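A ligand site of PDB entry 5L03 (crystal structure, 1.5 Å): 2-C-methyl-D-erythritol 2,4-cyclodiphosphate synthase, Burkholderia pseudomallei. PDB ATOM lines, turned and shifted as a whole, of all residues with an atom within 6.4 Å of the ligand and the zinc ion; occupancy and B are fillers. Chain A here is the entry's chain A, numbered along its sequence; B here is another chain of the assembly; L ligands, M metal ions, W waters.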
ATOM      1  N   ASP A  10       2.407 -26.688  30.941  1.00  0.00           N
ATOM      2  CA  ASP A  10       3.103 -27.377  29.862  1.00  0.00           C
ATOM      3  C   ASP A  10       2.260 -28.559  29.396  1.00  0.00           C
ATOM      4  O   ASP A  10       1.426 -29.089  30.126  1.00  0.00           O
ATOM      5  CB  ASP A  10       4.515 -27.779  30.298  1.00  0.00           C
ATOM      6  CG  ASP A  10       5.414 -28.204  29.133  1.00  0.00           C
ATOM      7  OD1 ASP A  10       5.193 -27.728  27.988  1.00  0.00           O
ATOM      8  OD2 ASP A  10       6.397 -28.932  29.373  1.00  0.00           O
ATOM      9  N   VAL A  11       2.501 -28.953  28.152  1.00  0.00           N
ATOM     10  CA  VAL A  11       1.863 -30.126  27.581  1.00  0.00           C
ATOM     11  C   VAL A  11       2.852 -30.738  26.597  1.00  0.00           C
ATOM     12  O   VAL A  11       3.597 -30.027  25.924  1.00  0.00           O
ATOM     13  CB  VAL A  11       0.504 -29.788  26.910  1.00  0.00           C
ATOM     14  CG1 VAL A  11       0.704 -28.947  25.652  1.00  0.00           C
ATOM     15  CG2 VAL A  11      -0.292 -31.073  26.628  1.00  0.00           C
ATOM     16  N   HIS A  12       2.858 -32.074  26.537  1.00  0.00           N
ATOM     17  CA  HIS A  12       3.641 -32.780  25.532  1.00  0.00           C
ATOM     18  C   HIS A  12       2.841 -33.950  25.005  1.00  0.00           C
ATOM     19  O   HIS A  12       2.033 -34.540  25.731  1.00  0.00           O
ATOM     20  CB  HIS A  12       4.945 -33.364  26.124  1.00  0.00           C
ATOM     21  CG  HIS A  12       5.993 -32.334  26.407  1.00  0.00           C
ATOM     22  ND1 HIS A  12       7.006 -32.035  25.511  1.00  0.00           N
ATOM     23  CD2 HIS A  12       6.198 -31.539  27.476  1.00  0.00           C
ATOM     24  CE1 HIS A  12       7.770 -31.095  26.017  1.00  0.00           C
ATOM     25  NE2 HIS A  12       7.314 -30.783  27.213  1.00  0.00           N
ATOM     26  N   LEU A  34       7.187 -36.544  24.063  1.00  0.00           N
ATOM     27  CA  LEU A  34       7.986 -36.128  22.910  1.00  0.00           C
ATOM     28  C   LEU A  34       8.464 -34.693  23.120  1.00  0.00           C
ATOM     29  O   LEU A  34       7.648 -33.794  23.374  1.00  0.00           O
ATOM     30  CB  LEU A  34       7.128 -36.192  21.643  1.00  0.00           C
ATOM     31  CG  LEU A  34       7.798 -35.649  20.384  1.00  0.00           C
ATOM     32  CD1 LEU A  34       9.085 -36.425  20.124  1.00  0.00           C
ATOM     33  CD2 LEU A  34       6.834 -35.756  19.216  1.00  0.00           C
ATOM     34  N   GLY A  35       9.766 -34.494  23.007  1.00  0.00           N
ATOM     35  CA  GLY A  35      10.321 -33.154  23.107  1.00  0.00           C
ATOM     36  C   GLY A  35      11.775 -33.183  22.714  1.00  0.00           C
ATOM     37  O   GLY A  35      12.357 -34.250  22.488  1.00  0.00           O
ATOM     38  N   HIS A  36      12.357 -31.986  22.595  1.00  0.00           N
ATOM     39  CA  HIS A  36      13.796 -31.886  22.373  1.00  0.00           C
ATOM     40  C   HIS A  36      14.567 -32.335  23.602  1.00  0.00           C
ATOM     41  O   HIS A  36      15.494 -33.154  23.509  1.00  0.00           O
ATOM     42  CB  HIS A  36      14.162 -30.446  22.002  1.00  0.00           C
ATOM     43  CG  HIS A  36      15.630 -30.213  21.783  1.00  0.00           C
ATOM     44  ND1 HIS A  36      16.319 -30.723  20.704  1.00  0.00           N
ATOM     45  CD2 HIS A  36      16.541 -29.511  22.515  1.00  0.00           C
ATOM     46  CE1 HIS A  36      17.588 -30.344  20.770  1.00  0.00           C
ATOM     47  NE2 HIS A  36      17.748 -29.613  21.859  1.00  0.00           N
ATOM     48  N   SER A  37      14.187 -31.822  24.767  1.00  0.00           N
ATOM     49  CA  SER A  37      14.714 -32.290  26.050  1.00  0.00           C
ATOM     50  C   SER A  37      14.114 -33.653  26.374  1.00  0.00           C
ATOM     51  O   SER A  37      13.500 -34.322  25.535  1.00  0.00           O
ATOM     52  CB  SER A  37      14.361 -31.293  27.134  1.00  0.00           C
ATOM     53  OG  SER A  37      12.956 -31.321  27.420  1.00  0.00           O
ATOM     54  N   ASP A  38      14.265 -34.076  27.637  1.00  0.00           N
ATOM     55  CA  ASP A  38      13.572 -35.286  28.075  1.00  0.00           C
ATOM     56  C   ASP A  38      12.056 -35.115  28.176  1.00  0.00           C
ATOM     57  O   ASP A  38      11.345 -36.076  28.504  1.00  0.00           O
ATOM     58  CB  ASP A  38      14.164 -35.822  29.392  1.00  0.00           C
ATOM     59  CG  ASP A  38      13.941 -34.912  30.596  1.00  0.00           C
ATOM     60  OD1 ASP A  38      13.141 -33.939  30.524  1.00  0.00           O
ATOM     61  OD2 ASP A  38      14.559 -35.196  31.656  1.00  0.00           O
ATOM     62  N   ALA A  39      11.549 -33.915  27.914  1.00  0.00           N
ATOM     63  CA  ALA A  39      10.118 -33.645  27.799  1.00  0.00           C
ATOM     64  C   ALA A  39       9.372 -33.816  29.121  1.00  0.00           C
ATOM     65  O   ALA A  39       8.175 -34.137  29.116  1.00  0.00           O
ATOM     66  CB  ALA A  39       9.451 -34.478  26.684  1.00  0.00           C
ATOM     67  N   ASP A  40      10.038 -33.548  30.245  1.00  0.00           N
ATOM     68  CA  ASP A  40       9.417 -33.664  31.562  1.00  0.00           C
ATOM     69  C   ASP A  40       8.418 -32.528  31.790  1.00  0.00           C
ATOM     70  O   ASP A  40       8.763 -31.441  32.248  1.00  0.00           O
ATOM     71  CB  ASP A  40      10.485 -33.680  32.657  1.00  0.00           C
ATOM     72  CG  ASP A  40       9.938 -34.143  33.987  1.00  0.00           C
ATOM     73  OD1 ASP A  40       8.779 -33.795  34.333  1.00  0.00           O
ATOM     74  OD2 ASP A  40      10.700 -34.802  34.717  1.00  0.00           O
ATOM     75  N   VAL A  41       7.164 -32.815  31.479  1.00  0.00           N
ATOM     76  CA  VAL A  41       6.115 -31.793  31.440  1.00  0.00           C
ATOM     77  C   VAL A  41       5.918 -31.152  32.808  1.00  0.00           C
ATOM     78  O   VAL A  41       5.640 -29.945  32.921  1.00  0.00           O
ATOM     79  CB  VAL A  41       4.834 -32.422  30.862  1.00  0.00           C
ATOM     80  CG1 VAL A  41       4.256 -33.493  31.788  1.00  0.00           C
ATOM     81  CG2 VAL A  41       3.786 -31.357  30.591  1.00  0.00           C
ATOM     82  N   HIS A  44       8.870 -28.808  33.632  1.00  0.00           N
ATOM     83  CA  HIS A  44       8.813 -27.598  32.808  1.00  0.00           C
ATOM     84  C   HIS A  44       7.764 -26.622  33.314  1.00  0.00           C
ATOM     85  O   HIS A  44       8.021 -25.408  33.355  1.00  0.00           O
ATOM     86  CB  HIS A  44       8.544 -27.932  31.347  1.00  0.00           C
ATOM     87  CG  HIS A  44       9.609 -28.737  30.712  1.00  0.00           C
ATOM     88  ND1 HIS A  44       9.473 -29.347  29.486  1.00  0.00           N
ATOM     89  CD2 HIS A  44      10.819 -29.130  31.200  1.00  0.00           C
ATOM     90  CE1 HIS A  44      10.565 -30.033  29.216  1.00  0.00           C
ATOM     91  NE2 HIS A  44      11.393 -29.928  30.241  1.00  0.00           N
ATOM     92  N   ALA A  45       6.582 -27.120  33.707  1.00  0.00           N
ATOM     93  CA  ALA A  45       5.578 -26.214  34.237  1.00  0.00           C
ATOM     94  C   ALA A  45       6.058 -25.544  35.510  1.00  0.00           C
ATOM     95  O   ALA A  45       5.837 -24.342  35.714  1.00  0.00           O
ATOM     96  CB  ALA A  45       4.289 -26.990  34.521  1.00  0.00           C
ATOM     97  N   ILE A  59      10.727 -20.410  30.223  1.00  0.00           N
ATOM     98  CA  ILE A  59      11.697 -21.487  30.067  1.00  0.00           C
ATOM     99  C   ILE A  59      12.335 -21.451  28.678  1.00  0.00           C
ATOM    100  O   ILE A  59      13.545 -21.711  28.522  1.00  0.00           O
ATOM    101  CB  ILE A  59      11.027 -22.845  30.388  1.00  0.00           C
ATOM    102  CG1 ILE A  59      12.089 -23.945  30.453  1.00  0.00           C
ATOM    103  CG2 ILE A  59       9.845 -23.114  29.422  1.00  0.00           C
ATOM    104  CD1 ILE A  59      11.545 -25.305  30.931  1.00  0.00           C
ATOM    105  N   GLY A  60      11.562 -21.067  27.658  1.00  0.00           N
ATOM    106  CA  GLY A  60      12.092 -20.984  26.302  1.00  0.00           C
ATOM    107  C   GLY A  60      13.129 -19.891  26.143  1.00  0.00           C
ATOM    108  O   GLY A  60      14.076 -20.040  25.366  1.00  0.00           O
ATOM    109  N   ARG A  61      12.976 -18.780  26.880  1.00  0.00           N
ATOM    110  CA  ARG A  61      13.976 -17.726  26.840  1.00  0.00           C
ATOM    111  C   ARG A  61      15.277 -18.189  27.473  1.00  0.00           C
ATOM    112  O   ARG A  61      16.360 -17.849  26.991  1.00  0.00           O
ATOM    113  CB  ARG A  61      13.457 -16.513  27.629  1.00  0.00           C
ATOM    114  CG  ARG A  61      14.514 -15.476  27.976  1.00  0.00           C
ATOM    115  CD  ARG A  61      13.910 -14.324  28.784  1.00  0.00           C
ATOM    116  NE  ARG A  61      14.868 -13.721  29.688  1.00  0.00           N
ATOM    117  CZ  ARG A  61      14.631 -12.653  30.436  1.00  0.00           C
ATOM    118  NH1 ARG A  61      13.443 -12.042  30.376  1.00  0.00           N
ATOM    119  NH2 ARG A  61      15.572 -12.182  31.248  1.00  0.00           N
ATOM    120  N   PHE A  63      16.441 -21.525  28.097  1.00  0.00           N
ATOM    121  CA  PHE A  63      17.083 -22.727  27.557  1.00  0.00           C
ATOM    122  C   PHE A  63      16.574 -22.896  26.139  1.00  0.00           C
ATOM    123  O   PHE A  63      15.368 -23.022  25.916  1.00  0.00           O
ATOM    124  CB  PHE A  63      16.708 -23.938  28.417  1.00  0.00           C
ATOM    125  CG  PHE A  63      16.926 -23.740  29.911  1.00  0.00           C
ATOM    126  CD1 PHE A  63      18.194 -23.590  30.445  1.00  0.00           C
ATOM    127  CD2 PHE A  63      15.846 -23.734  30.781  1.00  0.00           C
ATOM    128  CE1 PHE A  63      18.375 -23.410  31.804  1.00  0.00           C
ATOM    129  CE2 PHE A  63      16.025 -23.568  32.157  1.00  0.00           C
ATOM    130  CZ  PHE A  63      17.296 -23.404  32.651  1.00  0.00           C
ATOM    131  N   SER A  64      17.496 -22.903  25.171  1.00  0.00           N
ATOM    132  CA  SER A  64      17.114 -22.978  23.762  1.00  0.00           C
ATOM    133  C   SER A  64      16.692 -24.396  23.388  1.00  0.00           C
ATOM    134  O   SER A  64      17.493 -25.334  23.509  1.00  0.00           O
ATOM    135  CB  SER A  64      18.267 -22.527  22.881  1.00  0.00           C
ATOM    136  OG  SER A  64      17.986 -22.838  21.531  1.00  0.00           O
ATOM    137  N   ASP A  65      15.474 -24.541  22.874  1.00  0.00           N
ATOM    138  CA  ASP A  65      14.960 -25.850  22.480  1.00  0.00           C
ATOM    139  C   ASP A  65      15.518 -26.352  21.143  1.00  0.00           C
ATOM    140  O   ASP A  65      15.049 -27.371  20.641  1.00  0.00           O
ATOM    141  CB  ASP A  65      13.424 -25.874  22.476  1.00  0.00           C
ATOM    142  CG  ASP A  65      12.824 -24.897  21.467  1.00  0.00           C
ATOM    143  OD1 ASP A  65      13.567 -24.256  20.694  1.00  0.00           O
ATOM    144  OD2 ASP A  65      11.568 -24.789  21.463  1.00  0.00           O
ATOM    145  N   THR A  66      16.490 -25.649  20.562  1.00  0.00           N
ATOM    146  CA  THR A  66      17.195 -26.122  19.377  1.00  0.00           C
ATOM    147  C   THR A  66      18.703 -26.260  19.594  1.00  0.00           C
ATOM    148  O   THR A  66      19.412 -26.701  18.683  1.00  0.00           O
ATOM    149  CB  THR A  66      16.917 -25.216  18.167  1.00  0.00           C
ATOM    150  OG1 THR A  66      17.196 -23.845  18.509  1.00  0.00           O
ATOM    151  CG2 THR A  66      15.467 -25.349  17.726  1.00  0.00           C
ATOM    152  N   PHE A  70      21.012 -29.320  24.642  1.00  0.00           N
ATOM    153  CA  PHE A  70      19.801 -29.658  25.379  1.00  0.00           C
ATOM    154  C   PHE A  70      19.042 -30.835  24.777  1.00  0.00           C
ATOM    155  O   PHE A  70      17.950 -31.169  25.268  1.00  0.00           O
ATOM    156  CB  PHE A  70      18.862 -28.443  25.479  1.00  0.00           C
ATOM    157  CG  PHE A  70      19.409 -27.316  26.307  1.00  0.00           C
ATOM    158  CD1 PHE A  70      19.944 -27.551  27.566  1.00  0.00           C
ATOM    159  CD2 PHE A  70      19.408 -26.015  25.816  1.00  0.00           C
ATOM    160  CE1 PHE A  70      20.447 -26.510  28.324  1.00  0.00           C
ATOM    161  CE2 PHE A  70      19.911 -24.974  26.574  1.00  0.00           C
ATOM    162  CZ  PHE A  70      20.436 -25.213  27.824  1.00  0.00           C
ATOM    163  N   ALA A  73      18.041 -33.339  27.263  1.00  0.00           N
ATOM    164  CA  ALA A  73      18.478 -32.724  28.507  1.00  0.00           C
ATOM    165  C   ALA A  73      17.682 -33.231  29.704  1.00  0.00           C
ATOM    166  O   ALA A  73      16.457 -33.415  29.632  1.00  0.00           O
ATOM    167  CB  ALA A  73      18.340 -31.202  28.421  1.00  0.00           C
ATOM    168  N   SER A  75      15.746 -32.615  32.694  1.00  0.00           N
ATOM    169  CA  SER A  75      14.985 -31.448  33.118  1.00  0.00           C
ATOM    170  C   SER A  75      15.141 -31.138  34.602  1.00  0.00           C
ATOM    171  O   SER A  75      14.787 -30.028  35.029  1.00  0.00           O
ATOM    172  CB  SER A  75      13.519 -31.518  32.690  1.00  0.00           C
ATOM    173  OG  SER A  75      13.403 -31.522  31.268  1.00  0.00           O
ATOM    174  N   LEU A  78      17.831 -28.667  34.474  1.00  0.00           N
ATOM    175  CA  LEU A  78      17.265 -27.380  34.059  1.00  0.00           C
ATOM    176  C   LEU A  78      16.515 -26.719  35.208  1.00  0.00           C
ATOM    177  O   LEU A  78      16.616 -25.504  35.405  1.00  0.00           O
ATOM    178  CB  LEU A  78      16.336 -27.570  32.865  1.00  0.00           C
ATOM    179  CG  LEU A  78      17.016 -28.136  31.625  1.00  0.00           C
ATOM    180  CD1 LEU A  78      16.008 -28.150  30.478  1.00  0.00           C
ATOM    181  CD2 LEU A  78      18.269 -27.343  31.255  1.00  0.00           C
ATOM    182  N   LYS B 134       3.880 -19.994  24.983  1.00  0.00           N
ATOM    183  CA  LYS B 134       3.902 -21.433  24.784  1.00  0.00           C
ATOM    184  C   LYS B 134       3.156 -21.770  23.505  1.00  0.00           C
ATOM    185  O   LYS B 134       2.193 -21.092  23.144  1.00  0.00           O
ATOM    186  CB  LYS B 134       3.094 -22.135  25.898  1.00  0.00           C
ATOM    187  CG  LYS B 134       3.697 -22.080  27.283  1.00  0.00           C
ATOM    188  CD  LYS B 134       4.806 -23.093  27.328  1.00  0.00           C
ATOM    189  CE  LYS B 134       4.199 -24.483  27.163  1.00  0.00           C
ATOM    190  NZ  LYS B 134       5.160 -25.456  26.600  1.00  0.00           N
ATOM    191  N   GLU B 137       1.887 -27.764  21.386  1.00  0.00           N
ATOM    192  CA  GLU B 137       2.457 -29.001  20.830  1.00  0.00           C
ATOM    193  C   GLU B 137       1.483 -29.702  19.885  1.00  0.00           C
ATOM    194  O   GLU B 137       1.375 -30.927  19.872  1.00  0.00           O
ATOM    195  CB  GLU B 137       2.895 -29.932  21.973  1.00  0.00           C
ATOM    196  CG  GLU B 137       4.091 -29.421  22.776  1.00  0.00           C
ATOM    197  CD  GLU B 137       5.397 -29.440  22.012  1.00  0.00           C
ATOM    198  OE1 GLU B 137       6.245 -28.562  22.270  1.00  0.00           O
ATOM    199  OE2 GLU B 137       5.563 -30.308  21.134  1.00  0.00           O
HETATM  200  O1  LIG L   1      10.756 -27.795  24.760  1.00  0.00           O
HETATM  201  C1  LIG L   1      10.090 -27.972  25.762  1.00  0.00           C
HETATM  202  N1  LIG L   1      10.195 -29.322  26.355  1.00  0.00           N
HETATM  203  O2  LIG L   1      11.003 -30.221  25.711  1.00  0.00           O
HETATM  204  C2  LIG L   1       9.188 -26.838  26.436  1.00  0.00           C
HETATM  205  N2  LIG L   1       8.145 -27.506  27.122  1.00  0.00           N
HETATM  206  C3  LIG L   1      10.061 -26.014  27.365  1.00  0.00           C
HETATM  207  C4  LIG L   1      11.375 -25.690  26.824  1.00  0.00           C
HETATM  208  C5  LIG L   1      12.591 -26.407  27.014  1.00  0.00           C
HETATM  209  C6  LIG L   1      13.609 -25.702  26.264  1.00  0.00           C
HETATM  210  N3  LIG L   1      13.037 -24.591  25.624  1.00  0.00           N
HETATM  211  C7  LIG L   1      11.700 -24.611  25.984  1.00  0.00           C
HETATM  212  C8  LIG L   1      12.958 -27.548  27.714  1.00  0.00           C
HETATM  213  C9  LIG L   1      14.272 -27.979  27.686  1.00  0.00           C
HETATM  214  C10 LIG L   1      15.267 -27.290  26.967  1.00  0.00           C
HETATM  215  C11 LIG L   1      14.940 -26.160  26.249  1.00  0.00           C
HETATM  216 ZN    ZN M   1       7.977 -29.105  28.160  1.00  0.00          ZN
HETATM  217  O   HOH W   1      13.788 -22.493  23.449  1.00  0.00           O
HETATM  218  O   HOH W   2       8.189 -23.305  26.450  1.00  0.00           O
HETATM  219  O   HOH W   3       5.881 -28.158  25.224  1.00  0.00           O
HETATM  220  O   HOH W   4       9.977 -26.204  22.873  1.00  0.00           O
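Water W4 lies within hydrogen-bond range of OD2 of Asp 65 and O1 of the ligand. Water W1 lies within hydrogen-bond range of the backbone NH of Asp 65 (2.7 Å), the backbone carbonyl oxygen of Phe 63 (3.0 Å), a nitrogen (N3) of the ligand (3.1 Å) and the backbone carbonyl oxygen of Gly 60 (3.1 Å).
The side-chain hydroxyl (OG) of Ser 37 sits at hydrogen-bond distance from an oxygen (O2) of the ligand (2.8 Å). N3 of the ligand lies within hydrogen-bond range of O of Phe 63, 2.8 Å away.
The side-chain carboxylate (OD1) of Asp 10 is in salt-bridge range of the side-chain amino group (NZ) of Lys 134 of chain B (2.7 Å). A ring nitrogen (NE2) of His 44 sits at hydrogen-bond distance from the side-chain hydroxyl (OG) of Ser 75 (2.8 Å). A ring nitrogen (ND1) of His 12 lies within hydrogen-bond range of the backbone carbonyl oxygen (O) of Leu 34 (2.8 Å). The side-chain hydroxyl (OG) of Ser 37 sits at hydrogen-bond distance from the backbone NH (N) of Ala 39 (3.0 Å). OG1 of Thr 66 is in hydrogen-bond range of OG of Ser 64 (3.3 Å).
Gly 35 touches the ligand (CA to O2, 3.98 Å). N of His 36 touches O2 of the ligand, 3.8 Å away. Ile 59 touches the ligand. Gly 60 touches the ligand (CA to C7, 3.7 Å). C of Ser 64 touches C11 of the ligand, at 3.8 Å. Asp 65 touches the ligand (CB to N3, 3.4 Å). Leu 78 touches the ligand (CD1 to C9, 3.3 Å). Lys 134 of chain B touches the ligand. Hydrophobic or aromatic side chains within 4 Å of the ligand: His 12, His 44, Ile 59, Phe 63 and Leu 78. Of the 26 residues printed, 13 come within 4 Å of the ligand.
Of the 26 residues printed, 3 come within 4 Å of the zinc ion.
N2 of the ligand is bound to the zinc ion. OD2 of Asp 10 is bound to the zinc ion, at 2.0 Å. The zinc ion is bound by a ring nitrogen (ND1) of His 44. The zinc ion is bound by NE2 of His 12 (2.0 Å). The zinc ion has four donor atoms within binding distance.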
